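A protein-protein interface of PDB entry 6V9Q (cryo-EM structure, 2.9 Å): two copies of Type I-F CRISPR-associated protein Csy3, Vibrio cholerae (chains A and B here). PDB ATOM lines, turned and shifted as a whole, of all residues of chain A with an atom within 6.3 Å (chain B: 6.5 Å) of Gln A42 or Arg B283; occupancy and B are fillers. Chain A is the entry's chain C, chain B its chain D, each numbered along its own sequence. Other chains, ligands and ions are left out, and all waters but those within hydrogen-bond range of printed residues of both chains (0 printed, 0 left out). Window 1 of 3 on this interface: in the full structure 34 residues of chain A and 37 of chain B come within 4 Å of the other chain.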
ATOM      1  N   LEU A  40     -22.241  16.281  -5.518  1.00  0.00           N
ATOM      2  CA  LEU A  40     -22.903  17.017  -6.586  1.00  0.00           C
ATOM      3  C   LEU A  40     -22.665  16.271  -7.887  1.00  0.00           C
ATOM      4  O   LEU A  40     -21.529  16.176  -8.345  1.00  0.00           O
ATOM      5  CB  LEU A  40     -22.386  18.451  -6.659  1.00  0.00           C
ATOM      6  CG  LEU A  40     -23.008  19.435  -7.634  1.00  0.00           C
ATOM      7  CD1 LEU A  40     -23.069  20.747  -6.964  1.00  0.00           C
ATOM      8  CD2 LEU A  40     -22.141  19.584  -8.853  1.00  0.00           C
ATOM      9  N   GLY A  41     -23.730  15.747  -8.486  1.00  0.00           N
ATOM     10  CA  GLY A  41     -23.637  15.042  -9.739  1.00  0.00           C
ATOM     11  C   GLY A  41     -24.285  15.813 -10.874  1.00  0.00           C
ATOM     12  O   GLY A  41     -24.789  16.918 -10.713  1.00  0.00           O
ATOM     13  N   GLN A  42     -24.267  15.186 -12.046  1.00  0.00           N
ATOM     14  CA  GLN A  42     -25.002  15.701 -13.191  1.00  0.00           C
ATOM     15  C   GLN A  42     -26.487  15.415 -13.018  1.00  0.00           C
ATOM     16  O   GLN A  42     -26.948  14.883 -12.006  1.00  0.00           O
ATOM     17  CB  GLN A  42     -24.498  15.115 -14.502  1.00  0.00           C
ATOM     18  CG  GLN A  42     -23.364  15.843 -15.186  1.00  0.00           C
ATOM     19  CD  GLN A  42     -22.019  15.557 -14.607  1.00  0.00           C
ATOM     20  OE1 GLN A  42     -21.329  16.457 -14.134  1.00  0.00           O
ATOM     21  NE2 GLN A  42     -21.620  14.298 -14.660  1.00  0.00           N
ATOM     22  N   MET A  43     -27.253  15.733 -14.049  1.00  0.00           N
ATOM     23  CA  MET A  43     -28.695  15.690 -13.926  1.00  0.00           C
ATOM     24  C   MET A  43     -29.205  14.579 -14.836  1.00  0.00           C
ATOM     25  O   MET A  43     -30.172  14.757 -15.582  1.00  0.00           O
ATOM     26  CB  MET A  43     -29.273  17.075 -14.238  1.00  0.00           C
ATOM     27  CG  MET A  43     -30.657  17.322 -13.699  1.00  0.00           C
ATOM     28  SD  MET A  43     -31.187  19.025 -13.862  1.00  0.00           S
ATOM     29  CE  MET A  43     -30.249  19.786 -12.545  1.00  0.00           C
ATOM     30  N   GLU A  44     -28.544  13.423 -14.782  1.00  0.00           N
ATOM     31  CA  GLU A  44     -28.948  12.255 -15.553  1.00  0.00           C
ATOM     32  C   GLU A  44     -30.123  11.581 -14.870  1.00  0.00           C
ATOM     33  O   GLU A  44     -30.009  11.156 -13.716  1.00  0.00           O
ATOM     34  CB  GLU A  44     -27.832  11.226 -15.682  1.00  0.00           C
ATOM     35  CG  GLU A  44     -26.572  11.687 -16.328  1.00  0.00           C
ATOM     36  CD  GLU A  44     -25.423  11.837 -15.378  1.00  0.00           C
ATOM     37  OE1 GLU A  44     -25.581  11.514 -14.187  1.00  0.00           O
ATOM     38  OE2 GLU A  44     -24.339  12.245 -15.839  1.00  0.00           O
ATOM     39  N   LEU A  65     -30.207  21.705 -18.175  1.00  0.00           N
ATOM     40  CA  LEU A  65     -29.853  20.308 -18.027  1.00  0.00           C
ATOM     41  C   LEU A  65     -28.391  20.136 -17.639  1.00  0.00           C
ATOM     42  O   LEU A  65     -27.922  19.005 -17.499  1.00  0.00           O
ATOM     43  CB  LEU A  65     -30.176  19.574 -19.333  1.00  0.00           C
ATOM     44  CG  LEU A  65     -30.365  18.072 -19.465  1.00  0.00           C
ATOM     45  CD1 LEU A  65     -31.568  17.635 -18.674  1.00  0.00           C
ATOM     46  CD2 LEU A  65     -30.544  17.745 -20.920  1.00  0.00           C
ATOM     47  N   GLY A  68     -26.726  20.924 -12.096  1.00  0.00           N
ATOM     48  CA  GLY A  68     -26.125  20.404 -10.885  1.00  0.00           C
ATOM     49  C   GLY A  68     -27.139  19.833  -9.923  1.00  0.00           C
ATOM     50  O   GLY A  68     -28.023  20.549  -9.451  1.00  0.00           O
ATOM     51  N   ASN A  69     -27.013  18.549  -9.612  1.00  0.00           N
ATOM     52  CA  ASN A  69     -28.016  17.829  -8.829  1.00  0.00           C
ATOM     53  C   ASN A  69     -27.374  17.312  -7.550  1.00  0.00           C
ATOM     54  O   ASN A  69     -26.654  16.300  -7.581  1.00  0.00           O
ATOM     55  CB  ASN A  69     -28.589  16.678  -9.649  1.00  0.00           C
ATOM     56  CG  ASN A  69     -29.876  16.155  -9.091  1.00  0.00           C
ATOM     57  OD1 ASN A  69     -30.388  16.662  -8.096  1.00  0.00           O
ATOM     58  ND2 ASN A  69     -30.416  15.131  -9.726  1.00  0.00           N
ATOM     59  N   HIS A  71     -26.837  15.439  -3.965  1.00  0.00           N
ATOM     60  CA  HIS A  71     -27.322  14.266  -3.261  1.00  0.00           C
ATOM     61  C   HIS A  71     -26.548  14.150  -1.962  1.00  0.00           C
ATOM     62  O   HIS A  71     -25.640  14.932  -1.692  1.00  0.00           O
ATOM     63  CB  HIS A  71     -27.161  13.003  -4.107  1.00  0.00           C
ATOM     64  CG  HIS A  71     -27.910  13.042  -5.399  1.00  0.00           C
ATOM     65  ND1 HIS A  71     -29.279  12.925  -5.468  1.00  0.00           N
ATOM     66  CD2 HIS A  71     -27.479  13.179  -6.673  1.00  0.00           C
ATOM     67  CE1 HIS A  71     -29.661  12.992  -6.730  1.00  0.00           C
ATOM     68  NE2 HIS A  71     -28.587  13.145  -7.481  1.00  0.00           N
ATOM     69  N   PHE B 262     -15.241  10.974  -5.317  1.00  0.00           N
ATOM     70  CA  PHE B 262     -16.104  11.296  -6.480  1.00  0.00           C
ATOM     71  C   PHE B 262     -15.354  12.270  -7.392  1.00  0.00           C
ATOM     72  O   PHE B 262     -15.398  12.097  -8.617  1.00  0.00           O
ATOM     73  CB  PHE B 262     -17.456  11.822  -5.997  1.00  0.00           C
ATOM     74  CG  PHE B 262     -18.249  10.800  -5.226  1.00  0.00           C
ATOM     75  CD1 PHE B 262     -18.826   9.722  -5.871  1.00  0.00           C
ATOM     76  CD2 PHE B 262     -18.404  10.908  -3.855  1.00  0.00           C
ATOM     77  CE1 PHE B 262     -19.551   8.778  -5.163  1.00  0.00           C
ATOM     78  CE2 PHE B 262     -19.130   9.966  -3.148  1.00  0.00           C
ATOM     79  CZ  PHE B 262     -19.703   8.902  -3.803  1.00  0.00           C
ATOM     80  N   GLY B 265     -12.636  10.505  -9.471  1.00  0.00           N
ATOM     81  CA  GLY B 265     -13.195   9.766 -10.584  1.00  0.00           C
ATOM     82  C   GLY B 265     -13.658  10.638 -11.723  1.00  0.00           C
ATOM     83  O   GLY B 265     -13.705  10.174 -12.863  1.00  0.00           O
ATOM     84  N   ALA B 266     -14.001  11.891 -11.440  1.00  0.00           N
ATOM     85  CA  ALA B 266     -14.348  12.830 -12.492  1.00  0.00           C
ATOM     86  C   ALA B 266     -13.132  13.296 -13.268  1.00  0.00           C
ATOM     87  O   ALA B 266     -13.284  13.768 -14.392  1.00  0.00           O
ATOM     88  CB  ALA B 266     -15.074  14.031 -11.902  1.00  0.00           C
ATOM     89  N   ALA B 267     -11.937  13.179 -12.696  1.00  0.00           N
ATOM     90  CA  ALA B 267     -10.704  13.570 -13.362  1.00  0.00           C
ATOM     91  C   ALA B 267     -10.128  12.475 -14.229  1.00  0.00           C
ATOM     92  O   ALA B 267      -9.427  12.768 -15.199  1.00  0.00           O
ATOM     93  CB  ALA B 267      -9.644  13.950 -12.338  1.00  0.00           C
ATOM     94  N   ALA B 269     -12.011  10.402 -15.840  1.00  0.00           N
ATOM     95  CA  ALA B 269     -12.964  10.238 -16.926  1.00  0.00           C
ATOM     96  C   ALA B 269     -13.233  11.528 -17.692  1.00  0.00           C
ATOM     97  O   ALA B 269     -14.318  11.687 -18.250  1.00  0.00           O
ATOM     98  CB  ALA B 269     -14.267   9.666 -16.384  1.00  0.00           C
ATOM     99  N   THR B 270     -12.281  12.458 -17.739  1.00  0.00           N
ATOM    100  CA  THR B 270     -12.351  13.561 -18.698  1.00  0.00           C
ATOM    101  C   THR B 270     -11.704  13.077 -19.983  1.00  0.00           C
ATOM    102  O   THR B 270     -10.513  13.272 -20.224  1.00  0.00           O
ATOM    103  CB  THR B 270     -11.683  14.825 -18.181  1.00  0.00           C
ATOM    104  OG1 THR B 270     -10.354  14.519 -17.767  1.00  0.00           O
ATOM    105  CG2 THR B 270     -12.460  15.438 -17.052  1.00  0.00           C
ATOM    106  N   ILE B 271     -12.511  12.430 -20.815  1.00  0.00           N
ATOM    107  CA  ILE B 271     -12.056  11.691 -21.983  1.00  0.00           C
ATOM    108  C   ILE B 271     -12.849  12.067 -23.226  1.00  0.00           C
ATOM    109  O   ILE B 271     -12.326  12.033 -24.346  1.00  0.00           O
ATOM    110  CB  ILE B 271     -12.126  10.191 -21.645  1.00  0.00           C
ATOM    111  CG1 ILE B 271     -10.863   9.804 -20.918  1.00  0.00           C
ATOM    112  CG2 ILE B 271     -12.444   9.269 -22.811  1.00  0.00           C
ATOM    113  CD1 ILE B 271     -10.958   8.499 -20.410  1.00  0.00           C
ATOM    114  N   ASP B 272     -14.073  12.531 -23.021  1.00  0.00           N
ATOM    115  CA  ASP B 272     -15.036  12.743 -24.095  1.00  0.00           C
ATOM    116  C   ASP B 272     -14.624  13.947 -24.932  1.00  0.00           C
ATOM    117  O   ASP B 272     -14.953  15.088 -24.614  1.00  0.00           O
ATOM    118  CB  ASP B 272     -16.423  12.942 -23.501  1.00  0.00           C
ATOM    119  CG  ASP B 272     -17.520  12.890 -24.531  1.00  0.00           C
ATOM    120  OD1 ASP B 272     -17.248  12.603 -25.710  1.00  0.00           O
ATOM    121  OD2 ASP B 272     -18.675  13.161 -24.157  1.00  0.00           O
ATOM    122  N   PRO B 281     -11.620  18.029 -23.904  1.00  0.00           N
ATOM    123  CA  PRO B 281     -12.285  16.794 -23.470  1.00  0.00           C
ATOM    124  C   PRO B 281     -13.160  17.018 -22.246  1.00  0.00           C
ATOM    125  O   PRO B 281     -12.759  17.662 -21.277  1.00  0.00           O
ATOM    126  CB  PRO B 281     -11.120  15.849 -23.174  1.00  0.00           C
ATOM    127  CG  PRO B 281      -9.990  16.728 -22.899  1.00  0.00           C
ATOM    128  CD  PRO B 281     -10.161  17.934 -23.760  1.00  0.00           C
ATOM    129  N   LEU B 282     -14.365  16.475 -22.306  1.00  0.00           N
ATOM    130  CA  LEU B 282     -15.382  16.591 -21.278  1.00  0.00           C
ATOM    131  C   LEU B 282     -15.378  15.382 -20.360  1.00  0.00           C
ATOM    132  O   LEU B 282     -14.863  14.318 -20.697  1.00  0.00           O
ATOM    133  CB  LEU B 282     -16.756  16.737 -21.925  1.00  0.00           C
ATOM    134  CG  LEU B 282     -17.372  18.104 -22.158  1.00  0.00           C
ATOM    135  CD1 LEU B 282     -16.477  19.044 -22.929  1.00  0.00           C
ATOM    136  CD2 LEU B 282     -18.621  17.831 -22.955  1.00  0.00           C
ATOM    137  N   ARG B 283     -15.974  15.562 -19.187  1.00  0.00           N
ATOM    138  CA  ARG B 283     -16.189  14.446 -18.283  1.00  0.00           C
ATOM    139  C   ARG B 283     -17.274  13.551 -18.857  1.00  0.00           C
ATOM    140  O   ARG B 283     -18.292  14.035 -19.359  1.00  0.00           O
ATOM    141  CB  ARG B 283     -16.572  14.959 -16.897  1.00  0.00           C
ATOM    142  CG  ARG B 283     -16.501  13.944 -15.765  1.00  0.00           C
ATOM    143  CD  ARG B 283     -17.852  13.392 -15.362  1.00  0.00           C
ATOM    144  NE  ARG B 283     -17.775  12.544 -14.177  1.00  0.00           N
ATOM    145  CZ  ARG B 283     -17.525  11.241 -14.190  1.00  0.00           C
ATOM    146  NH1 ARG B 283     -17.337  10.609 -15.329  1.00  0.00           N
ATOM    147  NH2 ARG B 283     -17.477  10.568 -13.053  1.00  0.00           N
ATOM    148  N   VAL B 284     -17.027  12.242 -18.820  1.00  0.00           N
ATOM    149  CA  VAL B 284     -17.915  11.278 -19.453  1.00  0.00           C
ATOM    150  C   VAL B 284     -19.235  11.222 -18.703  1.00  0.00           C
ATOM    151  O   VAL B 284     -19.271  11.012 -17.486  1.00  0.00           O
ATOM    152  CB  VAL B 284     -17.254   9.894 -19.511  1.00  0.00           C
ATOM    153  CG1 VAL B 284     -18.243   8.874 -19.978  1.00  0.00           C
ATOM    154  CG2 VAL B 284     -16.078   9.909 -20.451  1.00  0.00           C
ATOM    155  N   GLY B 285     -20.325  11.433 -19.424  1.00  0.00           N
ATOM    156  CA  GLY B 285     -21.645  11.352 -18.834  1.00  0.00           C
ATOM    157  C   GLY B 285     -22.693  11.385 -19.917  1.00  0.00           C
ATOM    158  O   GLY B 285     -22.405  11.651 -21.084  1.00  0.00           O
ATOM    159  N   ARG B 286     -23.920  11.082 -19.510  1.00  0.00           N
ATOM    160  CA  ARG B 286     -25.068  11.268 -20.384  1.00  0.00           C
ATOM    161  C   ARG B 286     -25.245  12.745 -20.677  1.00  0.00           C
ATOM    162  O   ARG B 286     -25.062  13.583 -19.791  1.00  0.00           O
ATOM    163  CB  ARG B 286     -26.333  10.719 -19.732  1.00  0.00           C
ATOM    164  CG  ARG B 286     -26.575   9.260 -19.931  1.00  0.00           C
ATOM    165  CD  ARG B 286     -25.741   8.342 -19.069  1.00  0.00           C
ATOM    166  NE  ARG B 286     -26.169   8.251 -17.689  1.00  0.00           N
ATOM    167  CZ  ARG B 286     -25.466   7.633 -16.751  1.00  0.00           C
ATOM    168  NH1 ARG B 286     -25.924   7.562 -15.513  1.00  0.00           N
ATOM    169  NH2 ARG B 286     -24.316   7.055 -17.064  1.00  0.00           N
ATOM    170  N   PHE B 287     -25.630  13.048 -21.920  1.00  0.00           N
ATOM    171  CA  PHE B 287     -25.699  14.384 -22.520  1.00  0.00           C
ATOM    172  C   PHE B 287     -24.604  15.355 -22.103  1.00  0.00           C
ATOM    173  O   PHE B 287     -24.910  16.465 -21.675  1.00  0.00           O
ATOM    174  CB  PHE B 287     -27.090  15.035 -22.322  1.00  0.00           C
ATOM    175  CG  PHE B 287     -27.700  14.873 -20.958  1.00  0.00           C
ATOM    176  CD1 PHE B 287     -28.647  13.884 -20.743  1.00  0.00           C
ATOM    177  CD2 PHE B 287     -27.367  15.714 -19.911  1.00  0.00           C
ATOM    178  CE1 PHE B 287     -29.234  13.718 -19.512  1.00  0.00           C
ATOM    179  CE2 PHE B 287     -27.931  15.541 -18.662  1.00  0.00           C
ATOM    180  CZ  PHE B 287     -28.878  14.548 -18.470  1.00  0.00           C
ATOM    181  N   GLY B 288     -23.343  14.971 -22.336  1.00  0.00           N
ATOM    182  CA  GLY B 288     -22.141  15.482 -21.688  1.00  0.00           C
ATOM    183  C   GLY B 288     -22.005  16.968 -21.445  1.00  0.00           C
ATOM    184  O   GLY B 288     -21.898  17.762 -22.378  1.00  0.00           O
ATOM    185  N   VAL B 289     -21.994  17.347 -20.178  1.00  0.00           N
ATOM    186  CA  VAL B 289     -22.119  18.741 -19.811  1.00  0.00           C
ATOM    187  C   VAL B 289     -20.730  19.351 -19.710  1.00  0.00           C
ATOM    188  O   VAL B 289     -19.717  18.656 -19.592  1.00  0.00           O
ATOM    189  CB  VAL B 289     -22.902  18.918 -18.497  1.00  0.00           C
ATOM    190  CG1 VAL B 289     -24.125  18.049 -18.497  1.00  0.00           C
ATOM    191  CG2 VAL B 289     -22.048  18.645 -17.304  1.00  0.00           C
ATOM    192  N   PHE B 336     -18.089   6.319 -26.833  1.00  0.00           N
ATOM    193  CA  PHE B 336     -18.965   6.984 -25.877  1.00  0.00           C
ATOM    194  C   PHE B 336     -19.993   6.021 -25.310  1.00  0.00           C
ATOM    195  O   PHE B 336     -20.460   6.199 -24.183  1.00  0.00           O
ATOM    196  CB  PHE B 336     -19.639   8.171 -26.556  1.00  0.00           C
ATOM    197  CG  PHE B 336     -20.595   8.921 -25.680  1.00  0.00           C
ATOM    198  CD1 PHE B 336     -20.138   9.729 -24.660  1.00  0.00           C
ATOM    199  CD2 PHE B 336     -21.955   8.845 -25.908  1.00  0.00           C
ATOM    200  CE1 PHE B 336     -21.020  10.427 -23.870  1.00  0.00           C
ATOM    201  CE2 PHE B 336     -22.834   9.539 -25.122  1.00  0.00           C
ATOM    202  CZ  PHE B 336     -22.366  10.330 -24.104  1.00  0.00           C
ATOM    203  N   LYS B 343     -18.727   4.023 -16.668  1.00  0.00           N
ATOM    204  CA  LYS B 343     -19.160   5.005 -15.684  1.00  0.00           C
ATOM    205  C   LYS B 343     -20.298   4.465 -14.830  1.00  0.00           C
ATOM    206  O   LYS B 343     -20.407   4.823 -13.656  1.00  0.00           O
ATOM    207  CB  LYS B 343     -19.553   6.297 -16.404  1.00  0.00           C
ATOM    208  CG  LYS B 343     -19.762   7.516 -15.535  1.00  0.00           C
ATOM    209  CD  LYS B 343     -21.209   7.841 -15.357  1.00  0.00           C
ATOM    210  CE  LYS B 343     -21.385   9.081 -14.527  1.00  0.00           C
ATOM    211  NZ  LYS B 343     -20.895  10.294 -15.209  1.00  0.00           N
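No position is printed for both chains. Of the 6 pairs that touch across the chains among the printed residues, none has its exchanged pair printed and touching as well.
Gln A42 touches Arg B283 (NE2 to CD, 3.9 Å). Gln A42 touches Val B289 (CG to CG2, 3.8 Å). Met A43 touches Phe B287 (O to CZ, 3.2 Å). CB of Arg B286 touches CG of Glu A44, 3.5 Å away. CZ of Phe B287 touches CA of Glu A44, at 3.7 Å. CG of Leu A65 touches CE2 of Phe B287 (3.6 Å).
Hydrophobic or aromatic side chains of chain A that line the printed part of chain B: Leu A65. Among the printed residues, no Asp or Glu carboxylate lies within 4 Å of a Lys or Arg side-chain nitrogen of the other chain.
Printed residues of chain B within 4 Å of Glu A44: Arg B286 and Phe B287. Printed residues of chain B within 4 Å of Leu A65: Phe B287. Thr B270 touches none of the printed residues of chain A. Arg B283 touches one residue of chain A. Printed residues of chain A within 4 Å of Arg B286: Glu A44. The nearest residue of chain B that does not touch Gln A42 is Lys B343 (4.1 Å). The nearest printed residue of chain A that does not touch Arg B283 is Glu A44 (6.6 Å). The nearest printed residue of chain B that does not touch Leu A65 is Val B289 (4.04 Å).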
